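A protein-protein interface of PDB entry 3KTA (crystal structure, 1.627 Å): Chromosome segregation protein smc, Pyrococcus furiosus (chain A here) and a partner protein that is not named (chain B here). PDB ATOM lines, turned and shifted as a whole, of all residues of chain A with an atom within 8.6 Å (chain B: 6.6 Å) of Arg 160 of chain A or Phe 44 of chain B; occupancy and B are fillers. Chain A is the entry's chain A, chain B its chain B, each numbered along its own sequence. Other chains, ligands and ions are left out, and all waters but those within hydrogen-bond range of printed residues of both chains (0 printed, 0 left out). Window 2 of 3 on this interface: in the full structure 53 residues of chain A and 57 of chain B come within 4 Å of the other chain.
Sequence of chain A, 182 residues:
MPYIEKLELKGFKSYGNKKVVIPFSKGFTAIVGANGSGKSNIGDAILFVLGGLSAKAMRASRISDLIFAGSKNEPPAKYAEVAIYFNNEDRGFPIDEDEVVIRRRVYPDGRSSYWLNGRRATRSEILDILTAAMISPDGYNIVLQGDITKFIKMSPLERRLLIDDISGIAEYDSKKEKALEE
The guanidinium group (NH1) of Arg 160 of chain A sits at hydrogen-bond distance from the backbone carbonyl oxygen (O) of Gly 46 of chain B (3.0 Å). The guanidinium group of Arg 159 of chain A is in hydrogen-bond range of the backbone carbonyl oxygen of Leu 48 of chain B (2.7 Å). O of Pro 156 of chain A is in hydrogen-bond range of N of Leu 48 of chain B.
N of Leu 157 of chain A lies close to OG of Ser 155 of chain A (3.3 Å). OG of Ser 167 of chain A sits close to N of Ile 169 of chain A (3.4 Å). The backbone NH (N) of Phe 44 of chain B lies close to the side-chain carboxylate (OD1) of Asp 42 of chain B, at 3.4 Å. The backbone carbonyl oxygen (O) of Asp 164 of chain A lies within hydrogen-bond range of the side-chain hydroxyl (OG) of Ser 167 of chain A. The guanidinium group (NH2) of Arg 160 of chain A is in salt-bridge range of the side-chain carboxylate (OD2) of Asp 164 of chain A (2.8 Å). The backbone carbonyl oxygen (O) of Ile 163 of chain A sits close to the side-chain hydroxyl (OG) of Ser 167 of chain A.
Pro 156 of chain A touches Gly 47 of chain B (O to CA, 3.3 Å). CD1 of Leu 157 of chain A touches O of Gly 46 of chain B (3.8 Å). Arg 159 of chain A touches Phe 77 of chain B (CG to CZ, 3.7 Å). Arg 160 of chain A touches Phe 44 of chain B. Leu 162 of chain A touches Phe 77 of chain B. CG2 of Ile 163 of chain A touches CE1 of Phe 9 of chain B, 3.8 Å away. Ile 163 of chain A touches Leu 48 of chain B. Phe 9 of chain B touches Asp 164 of chain A (CE1 to OD1, 3.1 Å). Ser 167 of chain A touches Val 8 of chain B (O to CG1, 3.4 Å). Phe 44 of chain B touches Ile 169 of chain A (CE1 to CD1, 3.3 Å).
Of the printed residues of chain B, Pro 156 of chain A touches Gly 47 and Leu 48. Printed residues of chain B within 4 Å of Leu 157 of chain A: Gly 46 (3.8 Å) and Gly 47 (3.8 Å). Of chain B, only Phe 9, Pro 43, Phe 44, Gly 46 and Leu 48 come within 4 Å of Arg 160 of chain A. Of chain A, only Arg 160 (3.3 Å) comes within 4 Å of Pro 43 of chain B. No residue of chain A comes within 4 Å of Ser 45 of chain B. The nearest residue of chain B that does not touch Arg 160 of chain A is Gly 47 of chain B (4.1 Å). The nearest residue of chain A that does not touch Phe 44 of chain B is Asp 164 of chain A (4.2 Å).
Of the 15 printed residues of chain A, 9 touch a printed residue of chain B. Printed residues of chain A that touch a printed residue of chain B: Pro 156, Leu 157, Arg 159, Arg 160, Leu 162, Ile 163, Asp 164, Ser 167 and Ile 169. Of the 17 printed residues of chain B, 9 touch a printed residue of chain A. Along chain B the printed residues that touch a printed residue of chain A span positions 5 to 77. Among the printed residues, 19 pairs touch across the chains.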
ATOM      1  N   MET A 154       4.055  -9.405   5.149  1.00  0.00           N
ATOM      2  CA  MET A 154       2.738  -8.821   5.434  1.00  0.00           C
ATOM      3  C   MET A 154       2.853  -7.458   6.119  1.00  0.00           C
ATOM      4  O   MET A 154       3.843  -7.175   6.797  1.00  0.00           O
ATOM      5  CB  MET A 154       1.859  -9.783   6.255  1.00  0.00           C
ATOM      6  CG  MET A 154       2.423 -10.200   7.624  1.00  0.00           C
ATOM      7  SD  MET A 154       1.239 -11.414   8.629  1.00  0.00           S
ATOM      8  CE  MET A 154       0.977 -12.774   7.251  1.00  0.00           C
ATOM      9  N   SER A 155       1.847  -6.608   5.930  1.00  0.00           N
ATOM     10  CA  SER A 155       1.855  -5.292   6.572  1.00  0.00           C
ATOM     11  C   SER A 155       1.688  -5.462   8.069  1.00  0.00           C
ATOM     12  O   SER A 155       1.075  -6.436   8.513  1.00  0.00           O
ATOM     13  CB  SER A 155       0.713  -4.417   6.053  1.00  0.00           C
ATOM     14  OG  SER A 155      -0.534  -4.870   6.553  1.00  0.00           O
ATOM     15  N   PRO A 156       2.217  -4.510   8.856  1.00  0.00           N
ATOM     16  CA  PRO A 156       1.948  -4.514  10.295  1.00  0.00           C
ATOM     17  C   PRO A 156       0.465  -4.671  10.590  1.00  0.00           C
ATOM     18  O   PRO A 156       0.088  -5.347  11.543  1.00  0.00           O
ATOM     19  CB  PRO A 156       2.442  -3.136  10.732  1.00  0.00           C
ATOM     20  CG  PRO A 156       3.586  -2.865   9.805  1.00  0.00           C
ATOM     21  CD  PRO A 156       3.147  -3.429   8.476  1.00  0.00           C
ATOM     22  N   LEU A 157      -0.385  -4.067   9.767  1.00  0.00           N
ATOM     23  CA  LEU A 157      -1.821  -4.167  10.004  1.00  0.00           C
ATOM     24  C   LEU A 157      -2.331  -5.600   9.815  1.00  0.00           C
ATOM     25  O   LEU A 157      -3.067  -6.105  10.659  1.00  0.00           O
ATOM     26  CB  LEU A 157      -2.590  -3.181   9.120  1.00  0.00           C
ATOM     27  CG  LEU A 157      -4.042  -2.878   9.485  1.00  0.00           C
ATOM     28  CD1 LEU A 157      -4.232  -2.637  10.977  1.00  0.00           C
ATOM     29  CD2 LEU A 157      -4.503  -1.659   8.700  1.00  0.00           C
ATOM     30  N   GLU A 158      -1.943  -6.254   8.717  1.00  0.00           N
ATOM     31  CA  GLU A 158      -2.318  -7.651   8.513  1.00  0.00           C
ATOM     32  C   GLU A 158      -1.804  -8.507   9.662  1.00  0.00           C
ATOM     33  O   GLU A 158      -2.473  -9.441  10.111  1.00  0.00           O
ATOM     34  CB  GLU A 158      -1.792  -8.197   7.177  1.00  0.00           C
ATOM     35  CG  GLU A 158      -2.010  -9.708   7.037  1.00  0.00           C
ATOM     36  CD  GLU A 158      -1.842 -10.223   5.622  1.00  0.00           C
ATOM     37  OE1 GLU A 158      -1.977 -11.449   5.430  1.00  0.00           O
ATOM     38  OE2 GLU A 158      -1.594  -9.413   4.707  1.00  0.00           O
ATOM     39  N   ARG A 159      -0.616  -8.182  10.151  1.00  0.00           N
ATOM     40  CA  ARG A 159      -0.035  -8.987  11.221  1.00  0.00           C
ATOM     41  C   ARG A 159      -0.858  -8.884  12.510  1.00  0.00           C
ATOM     42  O   ARG A 159      -1.087  -9.887  13.191  1.00  0.00           O
ATOM     43  CB  ARG A 159       1.431  -8.622  11.443  1.00  0.00           C
ATOM     44  CG  ARG A 159       2.164  -9.584  12.375  1.00  0.00           C
ATOM     45  CD  ARG A 159       3.657  -9.261  12.462  1.00  0.00           C
ATOM     46  NE  ARG A 159       4.324  -9.343  11.168  1.00  0.00           N
ATOM     47  CZ  ARG A 159       4.781  -8.294  10.488  1.00  0.00           C
ATOM     48  NH1 ARG A 159       4.653  -7.069  10.979  1.00  0.00           N
ATOM     49  NH2 ARG A 159       5.378  -8.471   9.318  1.00  0.00           N
ATOM     50  N   ARG A 160      -1.360  -7.690  12.828  1.00  0.00           N
ATOM     51  CA  ARG A 160      -2.160  -7.568  14.032  1.00  0.00           C
ATOM     52  C   ARG A 160      -3.475  -8.314  13.901  1.00  0.00           C
ATOM     53  O   ARG A 160      -3.977  -8.905  14.854  1.00  0.00           O
ATOM     54  CB  ARG A 160      -2.414  -6.105  14.399  1.00  0.00           C
ATOM     55  CG  ARG A 160      -2.883  -5.940  15.844  1.00  0.00           C
ATOM     56  CD  ARG A 160      -3.943  -4.846  15.962  1.00  0.00           C
ATOM     57  NE  ARG A 160      -5.227  -5.287  15.432  1.00  0.00           N
ATOM     58  CZ  ARG A 160      -5.900  -4.656  14.470  1.00  0.00           C
ATOM     59  NH1 ARG A 160      -5.413  -3.546  13.937  1.00  0.00           N
ATOM     60  NH2 ARG A 160      -7.067  -5.124  14.059  1.00  0.00           N
ATOM     61  N   LEU A 161      -4.048  -8.279  12.704  1.00  0.00           N
ATOM     62  CA  LEU A 161      -5.310  -8.947  12.473  1.00  0.00           C
ATOM     63  C   LEU A 161      -5.218 -10.456  12.702  1.00  0.00           C
ATOM     64  O   LEU A 161      -6.176 -11.084  13.149  1.00  0.00           O
ATOM     65  CB  LEU A 161      -5.797  -8.641  11.061  1.00  0.00           C
ATOM     66  CG  LEU A 161      -6.371  -7.234  10.991  1.00  0.00           C
ATOM     67  CD1 LEU A 161      -6.443  -6.830   9.539  1.00  0.00           C
ATOM     68  CD2 LEU A 161      -7.737  -7.213  11.653  1.00  0.00           C
ATOM     69  N   LEU A 162      -4.060 -11.027  12.391  1.00  0.00           N
ATOM     70  CA  LEU A 162      -3.806 -12.429  12.708  1.00  0.00           C
ATOM     71  C   LEU A 162      -3.927 -12.664  14.214  1.00  0.00           C
ATOM     72  O   LEU A 162      -4.562 -13.623  14.655  1.00  0.00           O
ATOM     73  CB  LEU A 162      -2.435 -12.858  12.178  1.00  0.00           C
ATOM     74  CG  LEU A 162      -2.023 -14.314  12.409  1.00  0.00           C
ATOM     75  CD1 LEU A 162      -3.110 -15.271  11.944  1.00  0.00           C
ATOM     76  CD2 LEU A 162      -0.706 -14.606  11.703  1.00  0.00           C
ATOM     77  N   ILE A 163      -3.339 -11.774  15.008  1.00  0.00           N
ATOM     78  CA  ILE A 163      -3.471 -11.881  16.454  1.00  0.00           C
ATOM     79  C   ILE A 163      -4.914 -11.654  16.939  1.00  0.00           C
ATOM     80  O   ILE A 163      -5.381 -12.349  17.839  1.00  0.00           O
ATOM     81  CB  ILE A 163      -2.457 -10.983  17.169  1.00  0.00           C
ATOM     82  CG1 ILE A 163      -1.045 -11.349  16.690  1.00  0.00           C
ATOM     83  CG2 ILE A 163      -2.610 -11.091  18.681  1.00  0.00           C
ATOM     84  CD1 ILE A 163      -0.747 -12.863  16.703  1.00  0.00           C
ATOM     85  N   ASP A 164      -5.634 -10.709  16.331  1.00  0.00           N
ATOM     86  CA  ASP A 164      -7.071 -10.573  16.609  1.00  0.00           C
ATOM     87  C   ASP A 164      -7.759 -11.924  16.496  1.00  0.00           C
ATOM     88  O   ASP A 164      -8.523 -12.322  17.374  1.00  0.00           O
ATOM     89  CB  ASP A 164      -7.746  -9.650  15.599  1.00  0.00           C
ATOM     90  CG  ASP A 164      -7.440  -8.197  15.820  1.00  0.00           C
ATOM     91  OD1 ASP A 164      -6.492  -7.877  16.565  1.00  0.00           O
ATOM     92  OD2 ASP A 164      -8.164  -7.371  15.223  1.00  0.00           O
ATOM     93  N   ASP A 165      -7.484 -12.619  15.397  1.00  0.00           N
ATOM     94  CA  ASP A 165      -8.090 -13.914  15.124  1.00  0.00           C
ATOM     95  C   ASP A 165      -7.742 -14.933  16.205  1.00  0.00           C
ATOM     96  O   ASP A 165      -8.618 -15.600  16.750  1.00  0.00           O
ATOM     97  CB  ASP A 165      -7.665 -14.430  13.744  1.00  0.00           C
ATOM     98  CG  ASP A 165      -8.420 -15.679  13.336  1.00  0.00           C
ATOM     99  OD1 ASP A 165      -7.832 -16.780  13.386  1.00  0.00           O
ATOM    100  OD2 ASP A 165      -9.608 -15.559  12.976  1.00  0.00           O
ATOM    101  N   ILE A 166      -6.458 -15.043  16.524  1.00  0.00           N
ATOM    102  CA  ILE A 166      -6.010 -16.001  17.539  1.00  0.00           C
ATOM    103  C   ILE A 166      -6.647 -15.728  18.907  1.00  0.00           C
ATOM    104  O   ILE A 166      -6.985 -16.656  19.639  1.00  0.00           O
ATOM    105  CB  ILE A 166      -4.463 -16.002  17.651  1.00  0.00           C
ATOM    106  CG1 ILE A 166      -3.838 -16.361  16.297  1.00  0.00           C
ATOM    107  CG2 ILE A 166      -3.989 -16.976  18.709  1.00  0.00           C
ATOM    108  CD1 ILE A 166      -4.180 -17.761  15.783  1.00  0.00           C
ATOM    109  N   SER A 167      -6.817 -14.453  19.237  1.00  0.00           N
ATOM    110  CA  SER A 167      -7.349 -14.054  20.531  1.00  0.00           C
ATOM    111  C   SER A 167      -8.822 -14.445  20.678  1.00  0.00           C
ATOM    112  O   SER A 167      -9.345 -14.514  21.785  1.00  0.00           O
ATOM    113  CB  SER A 167      -7.178 -12.547  20.734  1.00  0.00           C
ATOM    114  OG  SER A 167      -8.092 -11.835  19.923  1.00  0.00           O
ATOM    115  N   ILE A 169     -11.372 -12.765  19.482  1.00  0.00           N
ATOM    116  CA  ILE A 169     -12.260 -11.610  19.400  1.00  0.00           C
ATOM    117  C   ILE A 169     -12.774 -11.438  17.979  1.00  0.00           C
ATOM    118  O   ILE A 169     -13.961 -11.196  17.771  1.00  0.00           O
ATOM    119  CB  ILE A 169     -11.570 -10.313  19.849  1.00  0.00           C
ATOM    120  CG1 ILE A 169     -10.541  -9.859  18.815  1.00  0.00           C
ATOM    121  CG2 ILE A 169     -10.913 -10.495  21.214  1.00  0.00           C
ATOM    122  CD1 ILE A 169      -9.672  -8.720  19.300  1.00  0.00           C
ATOM    123  N   LYS B   5     -12.943  -6.383  24.753  1.00  0.00           N
ATOM    124  CA  LYS B   5     -12.168  -6.951  23.653  1.00  0.00           C
ATOM    125  C   LYS B   5     -10.693  -6.582  23.787  1.00  0.00           C
ATOM    126  O   LYS B   5      -9.809  -7.384  23.461  1.00  0.00           O
ATOM    127  CB  LYS B   5     -12.722  -6.506  22.299  1.00  0.00           C
ATOM    128  CG  LYS B   5     -13.978  -7.259  21.885  1.00  0.00           C
ATOM    129  N   LYS B   6     -10.434  -5.372  24.275  1.00  0.00           N
ATOM    130  CA  LYS B   6      -9.072  -4.911  24.511  1.00  0.00           C
ATOM    131  C   LYS B   6      -8.364  -5.823  25.507  1.00  0.00           C
ATOM    132  O   LYS B   6      -7.179  -6.147  25.352  1.00  0.00           O
ATOM    133  CB  LYS B   6      -9.090  -3.486  25.060  1.00  0.00           C
ATOM    134  CG  LYS B   6      -7.742  -2.805  25.053  1.00  0.00           C
ATOM    135  CD  LYS B   6      -7.635  -1.820  26.206  1.00  0.00           C
ATOM    136  CE  LYS B   6      -6.552  -0.775  25.977  1.00  0.00           C
ATOM    137  NZ  LYS B   6      -5.279  -1.374  25.499  1.00  0.00           N
ATOM    138  N   ASN B   7      -9.103  -6.236  26.535  1.00  0.00           N
ATOM    139  CA  ASN B   7      -8.540  -7.077  27.589  1.00  0.00           C
ATOM    140  C   ASN B   7      -8.161  -8.463  27.091  1.00  0.00           C
ATOM    141  O   ASN B   7      -7.083  -8.968  27.414  1.00  0.00           O
ATOM    142  CB  ASN B   7      -9.507  -7.193  28.770  1.00  0.00           C
ATOM    143  CG  ASN B   7      -9.767  -5.858  29.444  1.00  0.00           C
ATOM    144  OD1 ASN B   7      -8.868  -5.027  29.588  1.00  0.00           O
ATOM    145  ND2 ASN B   7     -11.008  -5.651  29.870  1.00  0.00           N
ATOM    146  N   VAL B   8      -9.047  -9.082  26.316  1.00  0.00           N
ATOM    147  CA  VAL B   8      -8.758 -10.382  25.717  1.00  0.00           C
ATOM    148  C   VAL B   8      -7.578 -10.262  24.753  1.00  0.00           C
ATOM    149  O   VAL B   8      -6.681 -11.109  24.746  1.00  0.00           O
ATOM    150  CB  VAL B   8      -9.982 -10.979  24.984  1.00  0.00           C
ATOM    151  CG1 VAL B   8      -9.608 -12.305  24.316  1.00  0.00           C
ATOM    152  CG2 VAL B   8     -11.152 -11.176  25.953  1.00  0.00           C
ATOM    153  N   PHE B   9      -7.560  -9.198  23.954  1.00  0.00           N
ATOM    154  CA  PHE B   9      -6.461  -8.988  23.012  1.00  0.00           C
ATOM    155  C   PHE B   9      -5.130  -8.869  23.731  1.00  0.00           C
ATOM    156  O   PHE B   9      -4.167  -9.534  23.362  1.00  0.00           O
ATOM    157  CB  PHE B   9      -6.680  -7.757  22.126  1.00  0.00           C
ATOM    158  CG  PHE B   9      -5.556  -7.511  21.151  1.00  0.00           C
ATOM    159  CD1 PHE B   9      -5.570  -8.094  19.882  1.00  0.00           C
ATOM    160  CD2 PHE B   9      -4.483  -6.714  21.498  1.00  0.00           C
ATOM    161  CE1 PHE B   9      -4.530  -7.873  18.987  1.00  0.00           C
ATOM    162  CE2 PHE B   9      -3.434  -6.487  20.613  1.00  0.00           C
ATOM    163  CZ  PHE B   9      -3.455  -7.069  19.354  1.00  0.00           C
ATOM    164  N   MET B  10      -5.078  -8.022  24.754  1.00  0.00           N
ATOM    165  CA  MET B  10      -3.810  -7.760  25.437  1.00  0.00           C
ATOM    166  C   MET B  10      -3.233  -9.007  26.128  1.00  0.00           C
ATOM    167  O   MET B  10      -2.015  -9.207  26.147  1.00  0.00           O
ATOM    168  CB  MET B  10      -3.935  -6.563  26.390  1.00  0.00           C
ATOM    169  CG  MET B  10      -4.021  -5.200  25.651  1.00  0.00           C
ATOM    170  SD  MET B  10      -2.624  -4.876  24.375  1.00  0.00           S
ATOM    171  CE  MET B  10      -1.105  -5.423  25.464  1.00  0.00           C
ATOM    172  N   LEU B  37       3.389  -3.235  19.345  1.00  0.00           N
ATOM    173  CA  LEU B  37       2.130  -2.662  18.863  1.00  0.00           C
ATOM    174  C   LEU B  37       2.391  -1.228  18.420  1.00  0.00           C
ATOM    175  O   LEU B  37       2.975  -0.446  19.166  1.00  0.00           O
ATOM    176  CB  LEU B  37       1.062  -2.698  19.955  1.00  0.00           C
ATOM    177  CG  LEU B  37       0.542  -4.095  20.321  1.00  0.00           C
ATOM    178  CD1 LEU B  37      -0.331  -4.075  21.564  1.00  0.00           C
ATOM    179  CD2 LEU B  37      -0.218  -4.708  19.142  1.00  0.00           C
ATOM    180  N   ASN B  39       0.378   1.058  18.106  1.00  0.00           N
ATOM    181  CA  ASN B  39      -0.417   1.918  18.966  1.00  0.00           C
ATOM    182  C   ASN B  39      -0.837   1.174  20.232  1.00  0.00           C
ATOM    183  O   ASN B  39      -1.917   0.600  20.300  1.00  0.00           O
ATOM    184  CB  ASN B  39      -1.652   2.423  18.207  1.00  0.00           C
ATOM    185  CG  ASN B  39      -2.313   3.600  18.888  1.00  0.00           C
ATOM    186  OD1 ASN B  39      -2.519   3.596  20.101  1.00  0.00           O
ATOM    187  ND2 ASN B  39      -2.652   4.616  18.107  1.00  0.00           N
ATOM    188  N   GLU B  41      -1.855   2.185  23.149  1.00  0.00           N
ATOM    189  CA  GLU B  41      -3.055   2.703  23.811  1.00  0.00           C
ATOM    190  C   GLU B  41      -4.344   2.120  23.211  1.00  0.00           C
ATOM    191  O   GLU B  41      -5.260   1.701  23.936  1.00  0.00           O
ATOM    192  CB  GLU B  41      -3.069   4.234  23.727  1.00  0.00           C
ATOM    193  N   ASP B  42      -4.413   2.121  21.882  1.00  0.00           N
ATOM    194  CA  ASP B  42      -5.512   1.494  21.154  1.00  0.00           C
ATOM    195  C   ASP B  42      -4.926   0.652  20.035  1.00  0.00           C
ATOM    196  O   ASP B  42      -4.729   1.133  18.919  1.00  0.00           O
ATOM    197  CB  ASP B  42      -6.465   2.539  20.562  1.00  0.00           C
ATOM    198  CG  ASP B  42      -7.546   1.910  19.705  1.00  0.00           C
ATOM    199  OD1 ASP B  42      -7.834   0.711  19.909  1.00  0.00           O
ATOM    200  OD2 ASP B  42      -8.105   2.602  18.831  1.00  0.00           O
ATOM    201  N   PRO B  43      -4.617  -0.613  20.344  1.00  0.00           N
ATOM    202  CA  PRO B  43      -3.903  -1.503  19.426  1.00  0.00           C
ATOM    203  C   PRO B  43      -4.702  -1.653  18.159  1.00  0.00           C
ATOM    204  O   PRO B  43      -4.156  -1.768  17.065  1.00  0.00           O
ATOM    205  CB  PRO B  43      -3.887  -2.844  20.168  1.00  0.00           C
ATOM    206  CG  PRO B  43      -4.118  -2.512  21.603  1.00  0.00           C
ATOM    207  CD  PRO B  43      -5.009  -1.288  21.590  1.00  0.00           C
ATOM    208  N   PHE B  44      -6.016  -1.630  18.326  1.00  0.00           N
ATOM    209  CA  PHE B  44      -6.923  -1.823  17.214  1.00  0.00           C
ATOM    210  C   PHE B  44      -6.856  -0.659  16.213  1.00  0.00           C
ATOM    211  O   PHE B  44      -7.459  -0.733  15.141  1.00  0.00           O
ATOM    212  CB  PHE B  44      -8.340  -2.080  17.744  1.00  0.00           C
ATOM    213  CG  PHE B  44      -8.403  -3.205  18.762  1.00  0.00           C
ATOM    214  CD1 PHE B  44      -8.606  -4.509  18.358  1.00  0.00           C
ATOM    215  CD2 PHE B  44      -8.215  -2.959  20.113  1.00  0.00           C
ATOM    216  CE1 PHE B  44      -8.649  -5.538  19.279  1.00  0.00           C
ATOM    217  CE2 PHE B  44      -8.242  -4.002  21.040  1.00  0.00           C
ATOM    218  CZ  PHE B  44      -8.478  -5.275  20.625  1.00  0.00           C
ATOM    219  N   SER B  45      -6.099   0.389  16.557  1.00  0.00           N
ATOM    220  CA  SER B  45      -5.877   1.539  15.672  1.00  0.00           C
ATOM    221  C   SER B  45      -4.547   1.492  14.934  1.00  0.00           C
ATOM    222  O   SER B  45      -4.182   2.442  14.242  1.00  0.00           O
ATOM    223  CB  SER B  45      -5.943   2.857  16.459  1.00  0.00           C
ATOM    224  OG  SER B  45      -7.274   3.292  16.645  1.00  0.00           O
ATOM    225  N   GLY B  46      -3.808   0.396  15.081  1.00  0.00           N
ATOM    226  CA  GLY B  46      -2.475   0.323  14.514  1.00  0.00           C
ATOM    227  C   GLY B  46      -2.080  -1.111  14.206  1.00  0.00           C
ATOM    228  O   GLY B  46      -2.856  -2.026  14.438  1.00  0.00           O
ATOM    229  N   GLY B  47      -0.879  -1.287  13.664  1.00  0.00           N
ATOM    230  CA  GLY B  47      -0.394  -2.604  13.280  1.00  0.00           C
ATOM    231  C   GLY B  47       0.477  -3.260  14.338  1.00  0.00           C
ATOM    232  O   GLY B  47       0.604  -2.782  15.463  1.00  0.00           O
ATOM    233  N   LEU B  48       1.088  -4.373  13.965  1.00  0.00           N
ATOM    234  CA  LEU B  48       1.972  -5.082  14.875  1.00  0.00           C
ATOM    235  C   LEU B  48       3.303  -5.267  14.162  1.00  0.00           C
ATOM    236  O   LEU B  48       3.378  -5.918  13.111  1.00  0.00           O
ATOM    237  CB  LEU B  48       1.331  -6.413  15.292  1.00  0.00           C
ATOM    238  CG  LEU B  48       1.983  -7.265  16.385  1.00  0.00           C
ATOM    239  CD1 LEU B  48       0.989  -8.286  16.903  1.00  0.00           C
ATOM    240  CD2 LEU B  48       3.232  -7.948  15.865  1.00  0.00           C
ATOM    241  N   PHE B  77       7.759 -16.357  14.826  1.00  0.00           N
ATOM    242  CA  PHE B  77       6.406 -15.844  14.939  1.00  0.00           C
ATOM    243  C   PHE B  77       5.351 -16.957  14.890  1.00  0.00           C
ATOM    244  O   PHE B  77       4.434 -17.001  15.716  1.00  0.00           O
ATOM    245  CB  PHE B  77       6.169 -14.807  13.829  1.00  0.00           C
ATOM    246  CG  PHE B  77       4.848 -14.119  13.912  1.00  0.00           C
ATOM    247  CD1 PHE B  77       4.540 -13.291  14.978  1.00  0.00           C
ATOM    248  CD2 PHE B  77       3.913 -14.284  12.902  1.00  0.00           C
ATOM    249  CE1 PHE B  77       3.320 -12.656  15.054  1.00  0.00           C
ATOM    250  CE2 PHE B  77       2.684 -13.641  12.971  1.00  0.00           C
ATOM    251  CZ  PHE B  77       2.394 -12.821  14.046  1.00  0.00           C
